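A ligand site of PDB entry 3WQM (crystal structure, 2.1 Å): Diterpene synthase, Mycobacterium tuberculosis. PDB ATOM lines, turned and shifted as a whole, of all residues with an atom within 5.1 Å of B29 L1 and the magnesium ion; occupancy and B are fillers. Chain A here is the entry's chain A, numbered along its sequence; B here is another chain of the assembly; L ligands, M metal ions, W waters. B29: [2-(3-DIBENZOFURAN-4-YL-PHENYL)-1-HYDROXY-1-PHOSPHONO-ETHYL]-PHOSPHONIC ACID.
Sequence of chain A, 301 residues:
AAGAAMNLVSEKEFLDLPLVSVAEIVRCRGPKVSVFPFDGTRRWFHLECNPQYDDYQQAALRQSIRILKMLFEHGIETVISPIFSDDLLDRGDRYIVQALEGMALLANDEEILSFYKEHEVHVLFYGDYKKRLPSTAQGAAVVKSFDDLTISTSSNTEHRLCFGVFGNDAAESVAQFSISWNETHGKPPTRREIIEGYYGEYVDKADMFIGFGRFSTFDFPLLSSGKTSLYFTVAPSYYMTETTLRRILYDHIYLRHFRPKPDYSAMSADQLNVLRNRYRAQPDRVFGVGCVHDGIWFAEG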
ATOM      1  N   ASP A  39     -11.469 -10.344   5.863  1.00  0.00           N
ATOM      2  CA  ASP A  39     -11.226 -10.900   7.186  1.00  0.00           C
ATOM      3  C   ASP A  39     -12.558 -11.309   7.786  1.00  0.00           C
ATOM      4  O   ASP A  39     -13.617 -10.961   7.254  1.00  0.00           O
ATOM      5  CB  ASP A  39     -10.536  -9.847   8.055  1.00  0.00           C
ATOM      6  CG  ASP A  39      -9.880 -10.440   9.289  1.00  0.00           C
ATOM      7  OD1 ASP A  39      -9.256  -9.676  10.063  1.00  0.00           O
ATOM      8  OD2 ASP A  39      -9.984 -11.669   9.487  1.00  0.00           O
ATOM      9  N   GLY A  40     -12.514 -12.038   8.897  1.00  0.00           N
ATOM     10  CA  GLY A  40     -13.745 -12.484   9.525  1.00  0.00           C
ATOM     11  C   GLY A  40     -14.345 -13.648   8.744  1.00  0.00           C
ATOM     12  O   GLY A  40     -15.519 -13.941   8.858  1.00  0.00           O
ATOM     13  N   THR A  41     -13.513 -14.298   7.941  1.00  0.00           N
ATOM     14  CA  THR A  41     -13.933 -15.425   7.123  1.00  0.00           C
ATOM     15  C   THR A  41     -14.632 -16.536   7.927  1.00  0.00           C
ATOM     16  O   THR A  41     -15.752 -16.944   7.596  1.00  0.00           O
ATOM     17  CB  THR A  41     -12.735 -16.058   6.395  1.00  0.00           C
ATOM     18  OG1 THR A  41     -11.857 -15.038   5.920  1.00  0.00           O
ATOM     19  CG2 THR A  41     -13.212 -16.903   5.220  1.00  0.00           C
ATOM     20  N   ARG A  42     -13.968 -17.013   8.972  1.00  0.00           N
ATOM     21  CA  ARG A  42     -14.510 -18.068   9.810  1.00  0.00           C
ATOM     22  C   ARG A  42     -15.869 -17.765  10.429  1.00  0.00           C
ATOM     23  O   ARG A  42     -16.802 -18.552  10.309  1.00  0.00           O
ATOM     24  CB  ARG A  42     -13.526 -18.414  10.927  1.00  0.00           C
ATOM     25  CG  ARG A  42     -12.664 -19.634  10.656  1.00  0.00           C
ATOM     26  CD  ARG A  42     -11.593 -19.735  11.727  1.00  0.00           C
ATOM     27  NE  ARG A  42     -11.151 -21.104  11.989  1.00  0.00           N
ATOM     28  CZ  ARG A  42     -10.197 -21.419  12.866  1.00  0.00           C
ATOM     29  NH1 ARG A  42      -9.581 -20.464  13.545  1.00  0.00           N
ATOM     30  NH2 ARG A  42      -9.867 -22.688  13.061  1.00  0.00           N
ATOM     31  N   ARG A  43     -15.992 -16.612  11.090  1.00  0.00           N
ATOM     32  CA  ARG A  43     -17.245 -16.261  11.729  1.00  0.00           C
ATOM     33  C   ARG A  43     -18.347 -15.990  10.715  1.00  0.00           C
ATOM     34  O   ARG A  43     -19.520 -16.276  10.974  1.00  0.00           O
ATOM     35  CB  ARG A  43     -17.057 -15.053  12.656  1.00  0.00           C
ATOM     36  CG  ARG A  43     -17.088 -13.708  11.986  1.00  0.00           C
ATOM     37  CD  ARG A  43     -16.511 -12.681  12.924  1.00  0.00           C
ATOM     38  NE  ARG A  43     -15.058 -12.797  12.991  1.00  0.00           N
ATOM     39  CZ  ARG A  43     -14.268 -12.007  13.699  1.00  0.00           C
ATOM     40  NH1 ARG A  43     -14.792 -11.034  14.432  1.00  0.00           N
ATOM     41  NH2 ARG A  43     -12.956 -12.176  13.664  1.00  0.00           N
ATOM     42  N   TRP A  44     -17.989 -15.441   9.555  1.00  0.00           N
ATOM     43  CA  TRP A  44     -18.992 -15.177   8.539  1.00  0.00           C
ATOM     44  C   TRP A  44     -19.581 -16.506   8.091  1.00  0.00           C
ATOM     45  O   TRP A  44     -20.797 -16.689   8.081  1.00  0.00           O
ATOM     46  CB  TRP A  44     -18.378 -14.484   7.314  1.00  0.00           C
ATOM     47  CG  TRP A  44     -19.299 -14.529   6.122  1.00  0.00           C
ATOM     48  CD1 TRP A  44     -20.418 -13.777   5.922  1.00  0.00           C
ATOM     49  CD2 TRP A  44     -19.208 -15.412   5.003  1.00  0.00           C
ATOM     50  NE1 TRP A  44     -21.032 -14.134   4.740  1.00  0.00           N
ATOM     51  CE2 TRP A  44     -20.308 -15.138   4.155  1.00  0.00           C
ATOM     52  CE3 TRP A  44     -18.301 -16.417   4.631  1.00  0.00           C
ATOM     53  CZ2 TRP A  44     -20.525 -15.840   2.962  1.00  0.00           C
ATOM     54  CZ3 TRP A  44     -18.513 -17.108   3.430  1.00  0.00           C
ATOM     55  CH2 TRP A  44     -19.619 -16.810   2.617  1.00  0.00           C
ATOM     56  N   HIS A  46     -19.548 -19.619   9.485  1.00  0.00           N
ATOM     57  CA  HIS A  46     -20.315 -20.282  10.526  1.00  0.00           C
ATOM     58  C   HIS A  46     -21.586 -19.538  10.931  1.00  0.00           C
ATOM     59  O   HIS A  46     -22.500 -20.142  11.486  1.00  0.00           O
ATOM     60  CB  HIS A  46     -19.424 -20.490  11.755  1.00  0.00           C
ATOM     61  CG  HIS A  46     -18.280 -21.424  11.508  1.00  0.00           C
ATOM     62  ND1 HIS A  46     -18.447 -22.774  11.297  1.00  0.00           N
ATOM     63  CD2 HIS A  46     -16.944 -21.195  11.445  1.00  0.00           C
ATOM     64  CE1 HIS A  46     -17.267 -23.343  11.110  1.00  0.00           C
ATOM     65  NE2 HIS A  46     -16.334 -22.403  11.198  1.00  0.00           N
ATOM     66  N   LEU A  47     -21.652 -18.246  10.646  1.00  0.00           N
ATOM     67  CA  LEU A  47     -22.823 -17.448  11.003  1.00  0.00           C
ATOM     68  C   LEU A  47     -23.827 -17.240   9.867  1.00  0.00           C
ATOM     69  O   LEU A  47     -25.034 -17.251  10.098  1.00  0.00           O
ATOM     70  CB  LEU A  47     -22.397 -16.091  11.549  1.00  0.00           C
ATOM     71  CG  LEU A  47     -21.681 -16.075  12.901  1.00  0.00           C
ATOM     72  CD1 LEU A  47     -21.139 -14.683  13.206  1.00  0.00           C
ATOM     73  CD2 LEU A  47     -22.651 -16.523  13.995  1.00  0.00           C
ATOM     74  N   ARG A  91       0.344 -19.952  13.560  1.00  0.00           N
ATOM     75  CA  ARG A  91      -0.840 -20.756  13.812  1.00  0.00           C
ATOM     76  C   ARG A  91      -0.481 -22.206  13.463  1.00  0.00           C
ATOM     77  O   ARG A  91       0.630 -22.480  13.015  1.00  0.00           O
ATOM     78  CB  ARG A  91      -2.012 -20.260  12.966  1.00  0.00           C
ATOM     79  CG  ARG A  91      -2.689 -19.017  13.519  1.00  0.00           C
ATOM     80  CD  ARG A  91      -3.567 -19.350  14.716  1.00  0.00           C
ATOM     81  NE  ARG A  91      -4.360 -18.210  15.180  1.00  0.00           N
ATOM     82  CZ  ARG A  91      -5.254 -18.279  16.156  1.00  0.00           C
ATOM     83  NH1 ARG A  91      -5.473 -19.439  16.777  1.00  0.00           N
ATOM     84  NH2 ARG A  91      -5.939 -17.201  16.526  1.00  0.00           N
ATOM     85  N   TYR A  95      -3.536 -25.199   9.612  1.00  0.00           N
ATOM     86  CA  TYR A  95      -4.048 -23.853   9.371  1.00  0.00           C
ATOM     87  C   TYR A  95      -3.189 -23.207   8.280  1.00  0.00           C
ATOM     88  O   TYR A  95      -3.680 -22.466   7.438  1.00  0.00           O
ATOM     89  CB  TYR A  95      -3.954 -23.048  10.669  1.00  0.00           C
ATOM     90  CG  TYR A  95      -4.524 -21.647  10.643  1.00  0.00           C
ATOM     91  CD1 TYR A  95      -5.813 -21.385  11.110  1.00  0.00           C
ATOM     92  CD2 TYR A  95      -3.733 -20.569  10.259  1.00  0.00           C
ATOM     93  CE1 TYR A  95      -6.302 -20.081  11.203  1.00  0.00           C
ATOM     94  CE2 TYR A  95      -4.207 -19.256  10.350  1.00  0.00           C
ATOM     95  CZ  TYR A  95      -5.487 -19.030  10.826  1.00  0.00           C
ATOM     96  OH  TYR A  95      -5.933 -17.735  10.971  1.00  0.00           O
ATOM     97  N   ILE A 296     -15.918 -10.847  21.220  1.00  0.00           N
ATOM     98  CA  ILE A 296     -15.911  -9.997  20.040  1.00  0.00           C
ATOM     99  C   ILE A 296     -16.138  -8.539  20.425  1.00  0.00           C
ATOM    100  O   ILE A 296     -17.082  -8.203  21.143  1.00  0.00           O
ATOM    101  CB  ILE A 296     -16.972 -10.438  19.002  1.00  0.00           C
ATOM    102  CG1 ILE A 296     -16.678 -11.871  18.549  1.00  0.00           C
ATOM    103  CG2 ILE A 296     -16.932  -9.513  17.792  1.00  0.00           C
ATOM    104  CD1 ILE A 296     -17.730 -12.459  17.636  1.00  0.00           C
ATOM    105  N   TYR B 264     -15.130 -20.783  20.215  1.00  0.00           N
ATOM    106  CA  TYR B 264     -16.350 -20.588  19.445  1.00  0.00           C
ATOM    107  C   TYR B 264     -17.032 -21.865  18.986  1.00  0.00           C
ATOM    108  O   TYR B 264     -18.262 -21.918  18.881  1.00  0.00           O
ATOM    109  CB  TYR B 264     -16.059 -19.694  18.253  1.00  0.00           C
ATOM    110  CG  TYR B 264     -15.628 -18.301  18.642  1.00  0.00           C
ATOM    111  CD1 TYR B 264     -16.557 -17.380  19.124  1.00  0.00           C
ATOM    112  CD2 TYR B 264     -14.290 -17.923  18.568  1.00  0.00           C
ATOM    113  CE1 TYR B 264     -16.155 -16.109  19.526  1.00  0.00           C
ATOM    114  CE2 TYR B 264     -13.879 -16.655  18.974  1.00  0.00           C
ATOM    115  CZ  TYR B 264     -14.821 -15.750  19.448  1.00  0.00           C
ATOM    116  OH  TYR B 264     -14.426 -14.500  19.854  1.00  0.00           O
ATOM    117  N   SER B 265     -16.245 -22.899  18.700  1.00  0.00           N
ATOM    118  CA  SER B 265     -16.818 -24.159  18.259  1.00  0.00           C
ATOM    119  C   SER B 265     -17.518 -24.825  19.439  1.00  0.00           C
ATOM    120  O   SER B 265     -18.166 -25.858  19.296  1.00  0.00           O
ATOM    121  CB  SER B 265     -15.728 -25.098  17.723  1.00  0.00           C
ATOM    122  OG  SER B 265     -14.776 -25.410  18.721  1.00  0.00           O
ATOM    123  N   LEU B 272     -24.380 -18.275  19.564  1.00  0.00           N
ATOM    124  CA  LEU B 272     -24.026 -18.058  18.176  1.00  0.00           C
ATOM    125  C   LEU B 272     -25.183 -17.420  17.424  1.00  0.00           C
ATOM    126  O   LEU B 272     -24.996 -16.830  16.361  1.00  0.00           O
ATOM    127  CB  LEU B 272     -23.621 -19.373  17.526  1.00  0.00           C
ATOM    128  CG  LEU B 272     -22.400 -20.060  18.166  1.00  0.00           C
ATOM    129  CD1 LEU B 272     -22.112 -21.354  17.435  1.00  0.00           C
ATOM    130  CD2 LEU B 272     -21.179 -19.139  18.101  1.00  0.00           C
ATOM    131  N   LEU B 275     -25.255 -13.645  18.493  1.00  0.00           N
ATOM    132  CA  LEU B 275     -24.136 -13.035  17.786  1.00  0.00           C
ATOM    133  C   LEU B 275     -24.525 -12.767  16.345  1.00  0.00           C
ATOM    134  O   LEU B 275     -24.297 -11.683  15.815  1.00  0.00           O
ATOM    135  CB  LEU B 275     -22.915 -13.967  17.827  1.00  0.00           C
ATOM    136  CG  LEU B 275     -21.700 -13.536  17.003  1.00  0.00           C
ATOM    137  CD1 LEU B 275     -21.158 -12.204  17.518  1.00  0.00           C
ATOM    138  CD2 LEU B 275     -20.615 -14.618  17.082  1.00  0.00           C
HETATM  139  CAY B29 L   1     -16.803 -21.706  14.747  1.00  0.00           C
HETATM  140  CAP B29 L   1     -17.346 -23.019  14.641  1.00  0.00           C
HETATM  141  CAI B29 L   1     -16.486 -24.134  14.507  1.00  0.00           C
HETATM  142  CAH B29 L   1     -15.077 -23.948  14.479  1.00  0.00           C
HETATM  143  CAO B29 L   1     -14.534 -22.634  14.585  1.00  0.00           C
HETATM  144  CAX B29 L   1     -15.398 -21.521  14.729  1.00  0.00           C
HETATM  145  OAT B29 L   1     -15.155 -20.185  14.850  1.00  0.00           O
HETATM  146  CBA B29 L   1     -16.333 -19.501  14.945  1.00  0.00           C
HETATM  147  CAZ B29 L   1     -17.387 -20.444  14.880  1.00  0.00           C
HETATM  148  CAQ B29 L   1     -18.733 -20.018  14.962  1.00  0.00           C
HETATM  149  CAK B29 L   1     -19.033 -18.646  15.104  1.00  0.00           C
HETATM  150  CAN B29 L   1     -17.995 -17.689  15.164  1.00  0.00           C
HETATM  151  CAW B29 L   1     -16.626 -18.091  15.096  1.00  0.00           C
HETATM  152  CAV B29 L   1     -15.570 -17.121  15.176  1.00  0.00           C
HETATM  153  CAR B29 L   1     -14.280 -17.345  14.593  1.00  0.00           C
HETATM  154  CAM B29 L   1     -15.794 -15.878  15.850  1.00  0.00           C
HETATM  155  CAJ B29 L   1     -14.770 -14.916  15.948  1.00  0.00           C
HETATM  156  CAL B29 L   1     -13.504 -15.152  15.387  1.00  0.00           C
HETATM  157  CAU B29 L   1     -13.246 -16.377  14.697  1.00  0.00           C
HETATM  158  CAS B29 L   1     -11.858 -16.672  14.070  1.00  0.00           C
HETATM  159  CBB B29 L   1     -11.139 -15.539  13.289  1.00  0.00           C
HETATM  160  PBC B29 L   1      -9.483 -16.178  12.661  1.00  0.00           P
HETATM  161  OAD B29 L   1      -9.657 -17.728  12.240  1.00  0.00           O
HETATM  162  OAE B29 L   1      -9.136 -15.384  11.313  1.00  0.00           O
HETATM  163  OAA B29 L   1      -8.412 -15.982  13.666  1.00  0.00           O
HETATM  164  PBD B29 L   1     -12.092 -14.910  11.788  1.00  0.00           P
HETATM  165  OAF B29 L   1     -11.756 -15.946  10.587  1.00  0.00           O
HETATM  166  OAG B29 L   1     -13.674 -15.001  12.040  1.00  0.00           O
HETATM  167  OAB B29 L   1     -11.649 -13.529  11.463  1.00  0.00           O
HETATM  168  OAC B29 L   1     -10.895 -14.434  14.169  1.00  0.00           O
HETATM  169  CAY B29 L   2      -9.913 -17.101   1.201  1.00  0.00           C
HETATM  170  CAP B29 L   2     -10.560 -16.704  -0.002  1.00  0.00           C
HETATM  171  CAI B29 L   2     -10.764 -15.328  -0.269  1.00  0.00           C
HETATM  172  CAH B29 L   2     -10.332 -14.354   0.662  1.00  0.00           C
HETATM  173  CAO B29 L   2      -9.691 -14.747   1.854  1.00  0.00           C
HETATM  174  CAX B29 L   2      -9.476 -16.116   2.126  1.00  0.00           C
HETATM  175  OAT B29 L   2      -8.896 -16.766   3.174  1.00  0.00           O
HETATM  176  CBA B29 L   2      -8.931 -18.121   2.965  1.00  0.00           C
HETATM  177  CAZ B29 L   2      -9.581 -18.342   1.721  1.00  0.00           C
HETATM  178  CAQ B29 L   2      -9.768 -19.666   1.240  1.00  0.00           C
HETATM  179  CAK B29 L   2      -9.307 -20.757   1.993  1.00  0.00           C
HETATM  180  CAN B29 L   2      -8.667 -20.566   3.239  1.00  0.00           C
HETATM  181  CAW B29 L   2      -8.459 -19.243   3.751  1.00  0.00           C
HETATM  182  CAV B29 L   2      -7.795 -19.061   5.017  1.00  0.00           C
HETATM  183  CAR B29 L   2      -7.491 -17.755   5.524  1.00  0.00           C
HETATM  184  CAM B29 L   2      -7.406 -20.189   5.810  1.00  0.00           C
HETATM  185  CAJ B29 L   2      -6.743 -20.003   7.054  1.00  0.00           C
HETATM  186  CAL B29 L   2      -6.458 -18.704   7.519  1.00  0.00           C
HETATM  187  CAU B29 L   2      -6.833 -17.564   6.756  1.00  0.00           C
HETATM  188  CAS B29 L   2      -6.520 -16.139   7.241  1.00  0.00           C
HETATM  189  CBB B29 L   2      -7.390 -15.559   8.370  1.00  0.00           C
HETATM  190  PBC B29 L   2      -6.770 -13.839   8.769  1.00  0.00           P
HETATM  191  OAD B29 L   2      -7.465 -13.383  10.154  1.00  0.00           O
HETATM  192  OAE B29 L   2      -5.191 -13.947   9.058  1.00  0.00           O
HETATM  193  OAA B29 L   2      -7.041 -12.889   7.660  1.00  0.00           O
HETATM  194  PBD B29 L   2      -9.214 -15.421   7.934  1.00  0.00           P
HETATM  195  OAF B29 L   2      -9.275 -15.251   6.324  1.00  0.00           O
HETATM  196  OAG B29 L   2      -9.941 -16.810   8.298  1.00  0.00           O
HETATM  197  OAB B29 L   2      -9.831 -14.276   8.630  1.00  0.00           O
HETATM  198  OAC B29 L   2      -7.290 -16.383   9.523  1.00  0.00           O
HETATM  199 MG    MG M   1      -9.640 -13.360  10.891  1.00  0.00          MG
HETATM  200  O   HOH W   1      -9.000 -11.669  13.444  1.00  0.00           O
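Gly 40 touches the magnesium ion.
The backbone NH (N) of Arg 43 lies within hydrogen-bond range of an oxygen (OAG) of B29 L1 (3.0 Å).
NE of Arg 43 lies within salt-bridge range of OAG of B29 L1, 2.8 Å away.
OAF of B29 L1 is in hydrogen-bond range of N of Arg 42, 2.9 Å away.
An oxygen (OAD) of B29 L1 lies within salt-bridge range of the guanidinium group (NH1) of Arg 42.
OAB of B29 L1 sits close to N of Gly 40, at 3.1 Å.
OAA of B29 L1 is in salt-bridge range of NH2 of Arg 91, 3.97 Å away.
An oxygen (OAF) of B29 L2 is in hydrogen-bond range of the side-chain hydroxyl of Thr 41, at 2.6 Å.
OH of Tyr 95 is in hydrogen-bond range of OAC of B29 L2 (2.4 Å).
Residues that only touch B29 L1: His 46, Tyr 264 of chain B, Ser 265 of chain B, Thr 41, Leu 272 of chain B and Tyr 95.
Hydrophobic or aromatic side chains within 4 Å of B29 L1: His 46, Tyr 264 of chain B and Leu 272 of chain B.
Within 4 Å of B29 L1: Asp 39, Gly 40, Thr 41, Arg 42, Arg 43, His 46, Arg 91, Tyr 95, Tyr 264 of chain B, Ser 265 of chain B and Leu 272 of chain B.
Along chain A the residues within 4 Å of B29 L1 span positions 39 to 95.
The nearest printed residue that does not touch B29 L1 is Ile 296 (4.2 Å).
The magnesium ion is bound by an oxygen (OAB) of B29 L1 (2.1 Å), an oxygen (OAE) of B29 L1 (2.1 Å), the side-chain carboxylate of Asp 39 (2.2 Å), an oxygen (OAD) of B29 L2 (2.3 Å) and an oxygen (OAB) of B29 L2 (2.4 Å).
The magnesium ion has five donor atoms within binding distance.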
